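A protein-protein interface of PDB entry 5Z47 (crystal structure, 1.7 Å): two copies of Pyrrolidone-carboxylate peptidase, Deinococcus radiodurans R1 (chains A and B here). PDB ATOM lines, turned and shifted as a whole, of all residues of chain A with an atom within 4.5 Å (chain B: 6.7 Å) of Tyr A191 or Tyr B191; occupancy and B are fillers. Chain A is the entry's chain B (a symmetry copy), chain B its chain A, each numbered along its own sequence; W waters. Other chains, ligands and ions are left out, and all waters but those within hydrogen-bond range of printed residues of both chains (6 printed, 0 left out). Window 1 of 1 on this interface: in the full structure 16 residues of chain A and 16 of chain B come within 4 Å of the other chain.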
ATOM      1  N   PRO A  78      23.404  23.053 -18.556  1.00  0.00           N
ATOM      2  CA  PRO A  78      23.675  23.199 -19.999  1.00  0.00           C
ATOM      3  C   PRO A  78      22.796  22.344 -20.883  1.00  0.00           C
ATOM      4  O   PRO A  78      22.652  22.662 -22.073  1.00  0.00           O
ATOM      5  CB  PRO A  78      25.133  22.753 -20.127  1.00  0.00           C
ATOM      6  CG  PRO A  78      25.323  21.780 -18.999  1.00  0.00           C
ATOM      7  CD  PRO A  78      24.494  22.349 -17.852  1.00  0.00           C
ATOM      8  N   GLN A  79      22.236  21.258 -20.356  1.00  0.00           N
ATOM      9  CA  GLN A  79      21.540  20.287 -21.185  1.00  0.00           C
ATOM     10  C   GLN A  79      20.282  19.841 -20.461  1.00  0.00           C
ATOM     11  O   GLN A  79      20.182  19.940 -19.234  1.00  0.00           O
ATOM     12  CB  GLN A  79      22.432  19.072 -21.499  1.00  0.00           C
ATOM     13  CG  GLN A  79      23.832  19.457 -22.003  1.00  0.00           C
ATOM     14  CD  GLN A  79      24.741  18.272 -22.232  1.00  0.00           C
ATOM     15  OE1 GLN A  79      24.415  17.133 -21.839  1.00  0.00           O
ATOM     16  NE2 GLN A  79      25.876  18.514 -22.921  1.00  0.00           N
ATOM     17  N   ILE A 133      20.358  15.146 -29.276  1.00  0.00           N
ATOM     18  CA  ILE A 133      20.139  16.008 -28.115  1.00  0.00           C
ATOM     19  C   ILE A 133      20.973  15.471 -26.954  1.00  0.00           C
ATOM     20  O   ILE A 133      20.693  14.368 -26.448  1.00  0.00           O
ATOM     21  CB  ILE A 133      18.656  16.089 -27.728  1.00  0.00           C
ATOM     22  CG1 ILE A 133      17.838  16.663 -28.885  1.00  0.00           C
ATOM     23  CG2 ILE A 133      18.497  16.943 -26.468  1.00  0.00           C
ATOM     24  CD1 ILE A 133      16.332  16.551 -28.681  1.00  0.00           C
ATOM     25  N   PRO A 134      21.976  16.216 -26.485  1.00  0.00           N
ATOM     26  CA  PRO A 134      22.690  15.825 -25.258  1.00  0.00           C
ATOM     27  C   PRO A 134      21.770  15.897 -24.053  1.00  0.00           C
ATOM     28  O   PRO A 134      20.929  16.789 -23.954  1.00  0.00           O
ATOM     29  CB  PRO A 134      23.811  16.866 -25.139  1.00  0.00           C
ATOM     30  CG  PRO A 134      23.821  17.655 -26.372  1.00  0.00           C
ATOM     31  CD  PRO A 134      22.481  17.483 -27.047  1.00  0.00           C
ATOM     32  N   ALA A 174      18.006  27.391 -19.503  1.00  0.00           N
ATOM     33  CA  ALA A 174      17.573  28.709 -19.942  1.00  0.00           C
ATOM     34  C   ALA A 174      17.396  28.717 -21.453  1.00  0.00           C
ATOM     35  O   ALA A 174      18.125  28.031 -22.172  1.00  0.00           O
ATOM     36  CB  ALA A 174      18.624  29.754 -19.547  1.00  0.00           C
ATOM     37  N   ASN A 175      16.415  29.481 -21.934  1.00  0.00           N
ATOM     38  CA  ASN A 175      16.350  29.809 -23.356  1.00  0.00           C
ATOM     39  C   ASN A 175      17.081  31.138 -23.562  1.00  0.00           C
ATOM     40  O   ASN A 175      17.716  31.673 -22.643  1.00  0.00           O
ATOM     41  CB  ASN A 175      14.899  29.805 -23.872  1.00  0.00           C
ATOM     42  CG  ASN A 175      13.996  30.821 -23.161  1.00  0.00           C
ATOM     43  OD1 ASN A 175      14.463  31.675 -22.405  1.00  0.00           O
ATOM     44  ND2 ASN A 175      12.686  30.740 -23.433  1.00  0.00           N
ATOM     45  N   ALA A 176      17.024  31.672 -24.784  1.00  0.00           N
ATOM     46  CA  ALA A 176      17.709  32.923 -25.077  1.00  0.00           C
ATOM     47  C   ALA A 176      17.206  34.051 -24.179  1.00  0.00           C
ATOM     48  O   ALA A 176      18.008  34.822 -23.637  1.00  0.00           O
ATOM     49  CB  ALA A 176      17.527  33.282 -26.556  1.00  0.00           C
ATOM     50  N   ALA A 179      18.676  33.860 -20.703  1.00  0.00           N
ATOM     51  CA  ALA A 179      20.094  34.214 -20.703  1.00  0.00           C
ATOM     52  C   ALA A 179      20.307  35.707 -20.944  1.00  0.00           C
ATOM     53  O   ALA A 179      21.219  36.311 -20.365  1.00  0.00           O
ATOM     54  CB  ALA A 179      20.839  33.391 -21.756  1.00  0.00           C
ATOM     55  N   LEU A 189      24.915  32.465 -18.629  1.00  0.00           N
ATOM     56  CA  LEU A 189      24.240  31.190 -18.476  1.00  0.00           C
ATOM     57  C   LEU A 189      24.388  30.345 -19.729  1.00  0.00           C
ATOM     58  O   LEU A 189      24.231  30.862 -20.842  1.00  0.00           O
ATOM     59  CB  LEU A 189      22.747  31.395 -18.225  1.00  0.00           C
ATOM     60  CG  LEU A 189      22.279  31.950 -16.891  1.00  0.00           C
ATOM     61  CD1 LEU A 189      20.779  32.075 -16.965  1.00  0.00           C
ATOM     62  CD2 LEU A 189      22.704  31.033 -15.771  1.00  0.00           C
ATOM     63  N   PRO A 190      24.647  29.046 -19.592  1.00  0.00           N
ATOM     64  CA  PRO A 190      24.336  28.130 -20.695  1.00  0.00           C
ATOM     65  C   PRO A 190      22.876  28.307 -21.081  1.00  0.00           C
ATOM     66  O   PRO A 190      22.023  28.616 -20.249  1.00  0.00           O
ATOM     67  CB  PRO A 190      24.612  26.741 -20.109  1.00  0.00           C
ATOM     68  CG  PRO A 190      25.583  26.992 -18.983  1.00  0.00           C
ATOM     69  CD  PRO A 190      25.158  28.333 -18.409  1.00  0.00           C
ATOM     70  N   TYR A 191      22.591  28.130 -22.365  1.00  0.00           N
ATOM     71  CA  TYR A 191      21.228  28.310 -22.831  1.00  0.00           C
ATOM     72  C   TYR A 191      21.024  27.470 -24.078  1.00  0.00           C
ATOM     73  O   TYR A 191      21.969  26.989 -24.692  1.00  0.00           O
ATOM     74  CB  TYR A 191      20.916  29.795 -23.107  1.00  0.00           C
ATOM     75  CG  TYR A 191      21.421  30.306 -24.454  1.00  0.00           C
ATOM     76  CD1 TYR A 191      22.740  30.719 -24.617  1.00  0.00           C
ATOM     77  CD2 TYR A 191      20.562  30.383 -25.548  1.00  0.00           C
ATOM     78  CE1 TYR A 191      23.206  31.181 -25.860  1.00  0.00           C
ATOM     79  CE2 TYR A 191      21.005  30.847 -26.785  1.00  0.00           C
ATOM     80  CZ  TYR A 191      22.325  31.243 -26.933  1.00  0.00           C
ATOM     81  OH  TYR A 191      22.784  31.686 -28.150  1.00  0.00           O
ATOM     82  N   LEU A 192      19.759  27.297 -24.437  1.00  0.00           N
ATOM     83  CA  LEU A 192      19.370  26.673 -25.694  1.00  0.00           C
ATOM     84  C   LEU A 192      18.276  27.516 -26.321  1.00  0.00           C
ATOM     85  O   LEU A 192      17.434  28.066 -25.604  1.00  0.00           O
ATOM     86  CB  LEU A 192      18.861  25.240 -25.468  1.00  0.00           C
ATOM     87  CG  LEU A 192      19.915  24.274 -24.935  1.00  0.00           C
ATOM     88  CD1 LEU A 192      19.278  22.959 -24.576  1.00  0.00           C
ATOM     89  CD2 LEU A 192      21.033  24.064 -25.975  1.00  0.00           C
ATOM     90  N   PRO A 193      18.262  27.647 -27.643  1.00  0.00           N
ATOM     91  CA  PRO A 193      17.093  28.240 -28.295  1.00  0.00           C
ATOM     92  C   PRO A 193      15.840  27.487 -27.884  1.00  0.00           C
ATOM     93  O   PRO A 193      15.862  26.268 -27.684  1.00  0.00           O
ATOM     94  CB  PRO A 193      17.385  28.062 -29.790  1.00  0.00           C
ATOM     95  CG  PRO A 193      18.879  27.973 -29.868  1.00  0.00           C
ATOM     96  CD  PRO A 193      19.290  27.240 -28.617  1.00  0.00           C
ATOM     97  N   GLU A 196      14.985  24.221 -29.588  1.00  0.00           N
ATOM     98  CA  GLU A 196      15.713  23.037 -29.135  1.00  0.00           C
ATOM     99  C   GLU A 196      15.092  22.464 -27.868  1.00  0.00           C
ATOM    100  O   GLU A 196      14.972  21.245 -27.725  1.00  0.00           O
ATOM    101  CB  GLU A 196      17.186  23.379 -28.886  1.00  0.00           C
ATOM    102  CG  GLU A 196      18.022  22.253 -28.265  1.00  0.00           C
ATOM    103  CD  GLU A 196      18.441  21.183 -29.238  1.00  0.00           C
ATOM    104  OE1 GLU A 196      19.340  20.380 -28.896  1.00  0.00           O
ATOM    105  OE2 GLU A 196      17.901  21.144 -30.364  1.00  0.00           O
ATOM    106  N   ARG B  77      32.545  27.185 -23.561  1.00  0.00           N
ATOM    107  CA  ARG B  77      31.919  28.491 -23.430  1.00  0.00           C
ATOM    108  C   ARG B  77      30.428  28.386 -23.745  1.00  0.00           C
ATOM    109  O   ARG B  77      30.031  27.662 -24.669  1.00  0.00           O
ATOM    110  CB  ARG B  77      32.586  29.525 -24.352  1.00  0.00           C
ATOM    111  CG  ARG B  77      34.045  29.763 -24.021  1.00  0.00           C
ATOM    112  CD  ARG B  77      34.601  31.032 -24.665  1.00  0.00           C
ATOM    113  NE  ARG B  77      36.041  31.175 -24.398  1.00  0.00           N
ATOM    114  CZ  ARG B  77      36.798  32.151 -24.912  1.00  0.00           C
ATOM    115  NH1 ARG B  77      36.264  33.065 -25.706  1.00  0.00           N
ATOM    116  NH2 ARG B  77      38.106  32.206 -24.640  1.00  0.00           N
ATOM    117  N   PRO B  78      29.577  29.071 -22.979  1.00  0.00           N
ATOM    118  CA  PRO B  78      28.125  28.930 -23.193  1.00  0.00           C
ATOM    119  C   PRO B  78      27.575  29.804 -24.303  1.00  0.00           C
ATOM    120  O   PRO B  78      26.484  29.514 -24.814  1.00  0.00           O
ATOM    121  CB  PRO B  78      27.529  29.345 -21.846  1.00  0.00           C
ATOM    122  CG  PRO B  78      28.541  30.316 -21.285  1.00  0.00           C
ATOM    123  CD  PRO B  78      29.891  29.759 -21.716  1.00  0.00           C
ATOM    124  N   GLN B  79      28.260  30.884 -24.664  1.00  0.00           N
ATOM    125  CA  GLN B  79      27.707  31.852 -25.596  1.00  0.00           C
ATOM    126  C   GLN B  79      28.795  32.308 -26.551  1.00  0.00           C
ATOM    127  O   GLN B  79      29.985  32.254 -26.226  1.00  0.00           O
ATOM    128  CB  GLN B  79      27.108  33.058 -24.847  1.00  0.00           C
ATOM    129  CG  GLN B  79      26.181  32.644 -23.706  1.00  0.00           C
ATOM    130  CD  GLN B  79      25.645  33.818 -22.907  1.00  0.00           C
ATOM    131  OE1 GLN B  79      26.086  34.960 -23.090  1.00  0.00           O
ATOM    132  NE2 GLN B  79      24.683  33.541 -22.006  1.00  0.00           N
ATOM    133  N   VAL B  80      28.381  32.793 -27.728  1.00  0.00           N
ATOM    134  CA  VAL B  80      29.356  33.343 -28.669  1.00  0.00           C
ATOM    135  C   VAL B  80      30.105  34.502 -28.019  1.00  0.00           C
ATOM    136  O   VAL B  80      29.538  35.280 -27.240  1.00  0.00           O
ATOM    137  CB  VAL B  80      28.684  33.787 -29.984  1.00  0.00           C
ATOM    138  CG1 VAL B  80      28.249  32.591 -30.762  1.00  0.00           C
ATOM    139  CG2 VAL B  80      27.516  34.740 -29.722  1.00  0.00           C
ATOM    140  N   GLU B 132      18.356  38.577 -30.396  1.00  0.00           N
ATOM    141  CA  GLU B 132      18.091  37.684 -29.268  1.00  0.00           C
ATOM    142  C   GLU B 132      19.209  36.662 -29.057  1.00  0.00           C
ATOM    143  O   GLU B 132      18.947  35.551 -28.591  1.00  0.00           O
ATOM    144  CB  GLU B 132      16.742  36.968 -29.430  1.00  0.00           C
ATOM    145  CG  GLU B 132      15.544  37.908 -29.511  1.00  0.00           C
ATOM    146  CD  GLU B 132      15.266  38.577 -28.181  1.00  0.00           C
ATOM    147  OE1 GLU B 132      15.453  37.914 -27.136  1.00  0.00           O
ATOM    148  OE2 GLU B 132      14.868  39.761 -28.175  1.00  0.00           O
ATOM    149  N   ILE B 133      20.451  37.025 -29.375  1.00  0.00           N
ATOM    150  CA  ILE B 133      21.608  36.152 -29.183  1.00  0.00           C
ATOM    151  C   ILE B 133      22.425  36.674 -28.000  1.00  0.00           C
ATOM    152  O   ILE B 133      23.005  37.773 -28.075  1.00  0.00           O
ATOM    153  CB  ILE B 133      22.471  36.052 -30.446  1.00  0.00           C
ATOM    154  CG1 ILE B 133      21.638  35.513 -31.616  1.00  0.00           C
ATOM    155  CG2 ILE B 133      23.631  35.114 -30.214  1.00  0.00           C
ATOM    156  CD1 ILE B 133      22.321  35.603 -32.973  1.00  0.00           C
ATOM    157  N   PRO B 134      22.523  35.917 -26.905  1.00  0.00           N
ATOM    158  CA  PRO B 134      23.440  36.287 -25.817  1.00  0.00           C
ATOM    159  C   PRO B 134      24.880  36.217 -26.310  1.00  0.00           C
ATOM    160  O   PRO B 134      25.229  35.343 -27.095  1.00  0.00           O
ATOM    161  CB  PRO B 134      23.169  35.227 -24.740  1.00  0.00           C
ATOM    162  CG  PRO B 134      21.988  34.448 -25.168  1.00  0.00           C
ATOM    163  CD  PRO B 134      21.817  34.649 -26.651  1.00  0.00           C
ATOM    164  N   GLY B 135      25.717  37.143 -25.847  1.00  0.00           N
ATOM    165  CA  GLY B 135      27.119  37.111 -26.246  1.00  0.00           C
ATOM    166  C   GLY B 135      27.916  38.132 -25.466  1.00  0.00           C
ATOM    167  O   GLY B 135      27.358  38.961 -24.743  1.00  0.00           O
ATOM    168  N   PRO B 173      30.493  28.346 -29.171  1.00  0.00           N
ATOM    169  CA  PRO B 173      30.317  27.163 -28.316  1.00  0.00           C
ATOM    170  C   PRO B 173      30.372  25.872 -29.115  1.00  0.00           C
ATOM    171  O   PRO B 173      30.329  25.850 -30.351  1.00  0.00           O
ATOM    172  CB  PRO B 173      28.920  27.361 -27.721  1.00  0.00           C
ATOM    173  CG  PRO B 173      28.698  28.842 -27.753  1.00  0.00           C
ATOM    174  CD  PRO B 173      29.413  29.333 -28.998  1.00  0.00           C
ATOM    175  N   ALA B 174      30.442  24.772 -28.370  1.00  0.00           N
ATOM    176  CA  ALA B 174      30.172  23.452 -28.929  1.00  0.00           C
ATOM    177  C   ALA B 174      28.804  23.428 -29.601  1.00  0.00           C
ATOM    178  O   ALA B 174      27.863  24.090 -29.157  1.00  0.00           O
ATOM    179  CB  ALA B 174      30.205  22.403 -27.810  1.00  0.00           C
ATOM    180  N   ASN B 175      28.685  22.651 -30.672  1.00  0.00           N
ATOM    181  CA  ASN B 175      27.367  22.324 -31.200  1.00  0.00           C
ATOM    182  C   ASN B 175      26.927  21.000 -30.578  1.00  0.00           C
ATOM    183  O   ASN B 175      27.599  20.455 -29.696  1.00  0.00           O
ATOM    184  CB  ASN B 175      27.363  22.316 -32.736  1.00  0.00           C
ATOM    185  CG  ASN B 175      28.319  21.289 -33.340  1.00  0.00           C
ATOM    186  OD1 ASN B 175      28.854  20.420 -32.644  1.00  0.00           O
ATOM    187  ND2 ASN B 175      28.537  21.391 -34.659  1.00  0.00           N
ATOM    188  N   ALA B 176      25.793  20.466 -31.038  1.00  0.00           N
ATOM    189  CA  ALA B 176      25.285  19.219 -30.481  1.00  0.00           C
ATOM    190  C   ALA B 176      26.281  18.087 -30.672  1.00  0.00           C
ATOM    191  O   ALA B 176      26.504  17.287 -29.758  1.00  0.00           O
ATOM    192  CB  ALA B 176      23.944  18.860 -31.122  1.00  0.00           C
ATOM    193  N   ALA B 177      26.908  18.021 -31.848  1.00  0.00           N
ATOM    194  CA  ALA B 177      27.842  16.940 -32.131  1.00  0.00           C
ATOM    195  C   ALA B 177      29.011  16.950 -31.152  1.00  0.00           C
ATOM    196  O   ALA B 177      29.394  15.899 -30.619  1.00  0.00           O
ATOM    197  CB  ALA B 177      28.343  17.057 -33.572  1.00  0.00           C
ATOM    198  N   VAL B 178      29.593  18.131 -30.908  1.00  0.00           N
ATOM    199  CA  VAL B 178      30.699  18.237 -29.955  1.00  0.00           C
ATOM    200  C   VAL B 178      30.247  17.806 -28.567  1.00  0.00           C
ATOM    201  O   VAL B 178      30.931  17.031 -27.886  1.00  0.00           O
ATOM    202  CB  VAL B 178      31.277  19.666 -29.948  1.00  0.00           C
ATOM    203  CG1 VAL B 178      32.348  19.811 -28.847  1.00  0.00           C
ATOM    204  CG2 VAL B 178      31.850  20.019 -31.306  1.00  0.00           C
ATOM    205  N   ALA B 179      29.068  18.268 -28.136  1.00  0.00           N
ATOM    206  CA  ALA B 179      28.592  17.922 -26.804  1.00  0.00           C
ATOM    207  C   ALA B 179      28.295  16.427 -26.683  1.00  0.00           C
ATOM    208  O   ALA B 179      28.562  15.823 -25.644  1.00  0.00           O
ATOM    209  CB  ALA B 179      27.356  18.762 -26.463  1.00  0.00           C
ATOM    210  N   LEU B 189      28.978  19.630 -21.565  1.00  0.00           N
ATOM    211  CA  LEU B 189      29.330  20.924 -22.120  1.00  0.00           C
ATOM    212  C   LEU B 189      28.091  21.764 -22.392  1.00  0.00           C
ATOM    213  O   LEU B 189      27.090  21.254 -22.917  1.00  0.00           O
ATOM    214  CB  LEU B 189      30.096  20.761 -23.435  1.00  0.00           C
ATOM    215  CG  LEU B 189      31.523  20.221 -23.424  1.00  0.00           C
ATOM    216  CD1 LEU B 189      31.987  20.110 -24.856  1.00  0.00           C
ATOM    217  CD2 LEU B 189      32.418  21.146 -22.626  1.00  0.00           C
ATOM    218  N   PRO B 190      28.140  23.054 -22.088  1.00  0.00           N
ATOM    219  CA  PRO B 190      27.225  23.988 -22.753  1.00  0.00           C
ATOM    220  C   PRO B 190      27.339  23.797 -24.258  1.00  0.00           C
ATOM    221  O   PRO B 190      28.394  23.433 -24.772  1.00  0.00           O
ATOM    222  CB  PRO B 190      27.739  25.363 -22.322  1.00  0.00           C
ATOM    223  CG  PRO B 190      28.489  25.098 -21.022  1.00  0.00           C
ATOM    224  CD  PRO B 190      29.120  23.741 -21.223  1.00  0.00           C
ATOM    225  N   TYR B 191      26.234  24.003 -24.970  1.00  0.00           N
ATOM    226  CA  TYR B 191      26.242  23.832 -26.414  1.00  0.00           C
ATOM    227  C   TYR B 191      25.135  24.679 -27.019  1.00  0.00           C
ATOM    228  O   TYR B 191      24.254  25.180 -26.320  1.00  0.00           O
ATOM    229  CB  TYR B 191      26.082  22.355 -26.821  1.00  0.00           C
ATOM    230  CG  TYR B 191      24.655  21.851 -26.756  1.00  0.00           C
ATOM    231  CD1 TYR B 191      24.105  21.441 -25.548  1.00  0.00           C
ATOM    232  CD2 TYR B 191      23.883  21.728 -27.910  1.00  0.00           C
ATOM    233  CE1 TYR B 191      22.794  20.975 -25.474  1.00  0.00           C
ATOM    234  CE2 TYR B 191      22.583  21.264 -27.853  1.00  0.00           C
ATOM    235  CZ  TYR B 191      22.045  20.883 -26.635  1.00  0.00           C
ATOM    236  OH  TYR B 191      20.756  20.421 -26.591  1.00  0.00           O
ATOM    237  N   LEU B 192      25.199  24.839 -28.337  1.00  0.00           N
ATOM    238  CA  LEU B 192      24.138  25.467 -29.110  1.00  0.00           C
ATOM    239  C   LEU B 192      23.899  24.620 -30.345  1.00  0.00           C
ATOM    240  O   LEU B 192      24.851  24.060 -30.901  1.00  0.00           O
ATOM    241  CB  LEU B 192      24.490  26.890 -29.544  1.00  0.00           C
ATOM    242  CG  LEU B 192      24.685  27.874 -28.389  1.00  0.00           C
ATOM    243  CD1 LEU B 192      25.202  29.207 -28.881  1.00  0.00           C
ATOM    244  CD2 LEU B 192      23.375  28.080 -27.624  1.00  0.00           C
ATOM    245  N   PRO B 193      22.657  24.518 -30.801  1.00  0.00           N
ATOM    246  CA  PRO B 193      22.410  23.931 -32.122  1.00  0.00           C
ATOM    247  C   PRO B 193      23.229  24.668 -33.168  1.00  0.00           C
ATOM    248  O   PRO B 193      23.459  25.874 -33.062  1.00  0.00           O
ATOM    249  CB  PRO B 193      20.906  24.145 -32.337  1.00  0.00           C
ATOM    250  CG  PRO B 193      20.343  24.263 -30.934  1.00  0.00           C
ATOM    251  CD  PRO B 193      21.414  24.982 -30.159  1.00  0.00           C
ATOM    252  N   GLN B 194      23.685  23.925 -34.180  1.00  0.00           N
ATOM    253  CA  GLN B 194      24.516  24.550 -35.201  1.00  0.00           C
ATOM    254  C   GLN B 194      23.805  25.733 -35.859  1.00  0.00           C
ATOM    255  O   GLN B 194      24.449  26.730 -36.198  1.00  0.00           O
ATOM    256  CB  GLN B 194      24.949  23.517 -36.250  1.00  0.00           C
ATOM    257  CG  GLN B 194      25.849  24.111 -37.346  1.00  0.00           C
ATOM    258  CD  GLN B 194      27.180  24.574 -36.805  1.00  0.00           C
ATOM    259  OE1 GLN B 194      27.841  23.843 -36.058  1.00  0.00           O
ATOM    260  NE2 GLN B 194      27.593  25.799 -37.176  1.00  0.00           N
ATOM    261  N   GLU B 196      21.884  27.923 -34.533  1.00  0.00           N
ATOM    262  CA  GLU B 196      22.074  29.094 -33.682  1.00  0.00           C
ATOM    263  C   GLU B 196      23.477  29.663 -33.847  1.00  0.00           C
ATOM    264  O   GLU B 196      23.658  30.881 -33.899  1.00  0.00           O
ATOM    265  CB  GLU B 196      21.801  28.726 -32.221  1.00  0.00           C
ATOM    266  CG  GLU B 196      22.095  29.810 -31.195  1.00  0.00           C
ATOM    267  CD  GLU B 196      21.047  30.906 -31.140  1.00  0.00           C
ATOM    268  OE1 GLU B 196      21.057  31.681 -30.162  1.00  0.00           O
ATOM    269  OE2 GLU B 196      20.208  30.993 -32.062  1.00  0.00           O
ATOM    270  N   ILE B 197      24.482  28.786 -33.917  1.00  0.00           N
ATOM    271  CA  ILE B 197      25.866  29.223 -34.089  1.00  0.00           C
ATOM    272  C   ILE B 197      26.046  29.932 -35.428  1.00  0.00           C
ATOM    273  O   ILE B 197      26.638  31.019 -35.512  1.00  0.00           O
ATOM    274  CB  ILE B 197      26.804  28.010 -33.966  1.00  0.00           C
ATOM    275  CG1 ILE B 197      26.718  27.439 -32.544  1.00  0.00           C
ATOM    276  CG2 ILE B 197      28.245  28.414 -34.297  1.00  0.00           C
ATOM    277  CD1 ILE B 197      27.464  26.149 -32.346  1.00  0.00           C
ATOM    278  N   ARG B 199      23.836  31.350 -37.303  1.00  0.00           N
ATOM    279  CA  ARG B 199      23.129  32.624 -37.300  1.00  0.00           C
ATOM    280  C   ARG B 199      23.912  33.694 -36.543  1.00  0.00           C
ATOM    281  O   ARG B 199      23.937  34.857 -36.958  1.00  0.00           O
ATOM    282  CB  ARG B 199      21.735  32.451 -36.701  1.00  0.00           C
ATOM    283  CG  ARG B 199      20.920  33.722 -36.766  1.00  0.00           C
ATOM    284  CD  ARG B 199      19.458  33.459 -36.387  1.00  0.00           C
ATOM    285  NE  ARG B 199      19.310  33.098 -34.978  1.00  0.00           N
ATOM    286  CZ  ARG B 199      18.980  33.945 -34.006  1.00  0.00           C
ATOM    287  NH1 ARG B 199      18.738  35.232 -34.260  1.00  0.00           N
ATOM    288  NH2 ARG B 199      18.855  33.496 -32.768  1.00  0.00           N
ATOM    289  N   ALA B 200      24.581  33.321 -35.445  1.00  0.00           N
ATOM    290  CA  ALA B 200      25.377  34.311 -34.714  1.00  0.00           C
ATOM    291  C   ALA B 200      26.558  34.800 -35.541  1.00  0.00           C
ATOM    292  O   ALA B 200      26.869  35.997 -35.534  1.00  0.00           O
ATOM    293  CB  ALA B 200      25.868  33.745 -33.382  1.00  0.00           C
HETATM  294  O   HOH W   1      23.995  24.705 -23.337  1.00  0.00           O
HETATM  295  O   HOH W   2      23.546  35.133 -19.713  1.00  0.00           O
HETATM  296  O   HOH W   3      20.165  19.451 -24.075  1.00  0.00           O
HETATM  297  O   HOH W   4      28.438  16.993 -23.048  1.00  0.00           O
HETATM  298  O   HOH W   5      25.430  32.765 -27.823  1.00  0.00           O
HETATM  299  O   HOH W   6      24.924  27.462 -24.055  1.00  0.00           O
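Printed residues of chain B that touch a printed residue of chain A: Pro B78, Gln B79, Glu B132, Pro B134, Ala B179, Leu B189, Pro B190, Tyr B191, Leu B192, Pro B193 and Glu B196.
Hydrophobic or aromatic side chains of chain A that line the printed part of chain B: Pro A78, Pro A134, Ala A176, Ala A179, Tyr A191, Leu A192 and Pro A193.
Among the printed residues, no Asp or Glu carboxylate lies within 4 Å of a Lys or Arg side-chain nitrogen of the other chain.
Water W2 lies within hydrogen-bond range of the backbone carbonyl oxygen (O) of Ala A179 (2.7 Å), the side-chain amide nitrogen (NE2) of Gln B79 (3.0 Å) and the backbone NH (N) of Leu A189 (3.2 Å).
Water W1 lies within hydrogen-bond range of the backbone carbonyl oxygen of Pro A78 (2.8 Å), the backbone NH of Tyr B191 (2.9 Å) and the backbone carbonyl oxygen of Tyr A191 (3.3 Å).
Water W3 lies within hydrogen-bond range of the side-chain hydroxyl of Tyr B191 (2.8 Å) and the backbone carbonyl oxygen of Pro A134 (2.8 Å).
Water W4 lies within hydrogen-bond range of O of Ala B179 (2.9 Å), NE2 of Gln A79 (3.0 Å) and N of Leu B189 (3.1 Å).
O of Ala B174 is in hydrogen-bond range of N of Leu B192.
OE2 of Glu B196 lies within salt-bridge range of NH2 of Arg B199.
The backbone carbonyl oxygen of Ala A174 lies within hydrogen-bond range of the backbone NH of Leu A192 (2.9 Å).
Pro A134 touches Ala B179, and with the chains exchanged Ala A179 touches Pro B134.
Pro A134 touches Tyr B191, and with the chains exchanged Tyr A191 touches Pro B134.
Tyr A191 touches Leu B192, and with the chains exchanged Leu A192 touches Tyr B191.
Pro A193 touches Glu B196, and with the chains exchanged Glu A196 touches Pro B193.
Positions printed for both chains: 78, 79, 133, 134, 174, 175, 176, 179, 189, 190, 191, 192, 193 and 196.
Of the 25 pairs that touch across the chains among the printed residues, 24 have their exchanged pair printed and touching as well.
CE1 of Tyr B191 touches O of Pro A78 (3.8 Å).
Tyr B191 touches Gln A79 (CE1 to CG, 3.9 Å).
CG of Pro A134 touches CB of Ala B179, 3.7 Å away.
Glu B132 touches Ala A176.
CE1 of Tyr A191 touches O of Pro B78, 3.8 Å away.
Gln B79 touches Tyr A191 (CG to CE1, 3.95 Å).
CZ of Tyr A191 touches CD2 of Leu B192 (3.4 Å).
Tyr B191 touches Leu A192.
Pro A193 touches Pro B193 (CD to CD, 3.5 Å).
Pro A193 touches Glu B196.
Of chain B, only Pro B78, Gln B79, Pro B134, Tyr B191, Leu B192 and Glu B196 come within 4 Å of Tyr A191.
Of the printed residues of chain A, Tyr B191 touches Pro A78 (3.8 Å), Gln A79 (3.9 Å), Pro A134 (3.4 Å), Tyr A191 (3.3 Å), Leu A192 (3.4 Å) and Glu A196 (2.7 Å).
Printed residues of chain A within 4 Å of Leu B189: Pro A78 and Gln A79.
Printed residues of chain B within 4 Å of Gln A79: Ala B179 (3.8 Å), Leu B189 (3.0 Å) and Tyr B191 (3.9 Å).
Of the printed residues of chain B, Leu A189 touches Pro B78 (3.8 Å) and Gln B79 (3.0 Å).
Of the printed residues of chain A, Gln B79 touches Ala A179 (3.9 Å), Leu A189 (3.0 Å) and Tyr A191 (3.95 Å).
Arg B77 touches none of the printed residues of chain A.
The nearest residue of chain B that does not touch Tyr A191 is Ile B133 (4.1 Å).
The nearest residue of chain A that does not touch Tyr B191 is Ile A133 (4.1 Å).
The nearest printed residue of chain B that does not touch Ala A179 is Gly B135 (7.1 Å).
The side-chain amide nitrogen of Gln B79 is in hydrogen-bond range of the backbone carbonyl oxygen of Leu A189 (3.0 Å).
O of Leu B189 lies within hydrogen-bond range of NE2 of Gln A79 (3.0 Å).
OH of Tyr B191 lies within hydrogen-bond range of OE1 of Glu A196, at 2.7 Å.
The side-chain carboxylate of Glu B196 lies within hydrogen-bond range of the side-chain hydroxyl of Tyr A191, at 2.7 Å.
O of Tyr A191 sits close to O of Tyr B191 (3.3 Å).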
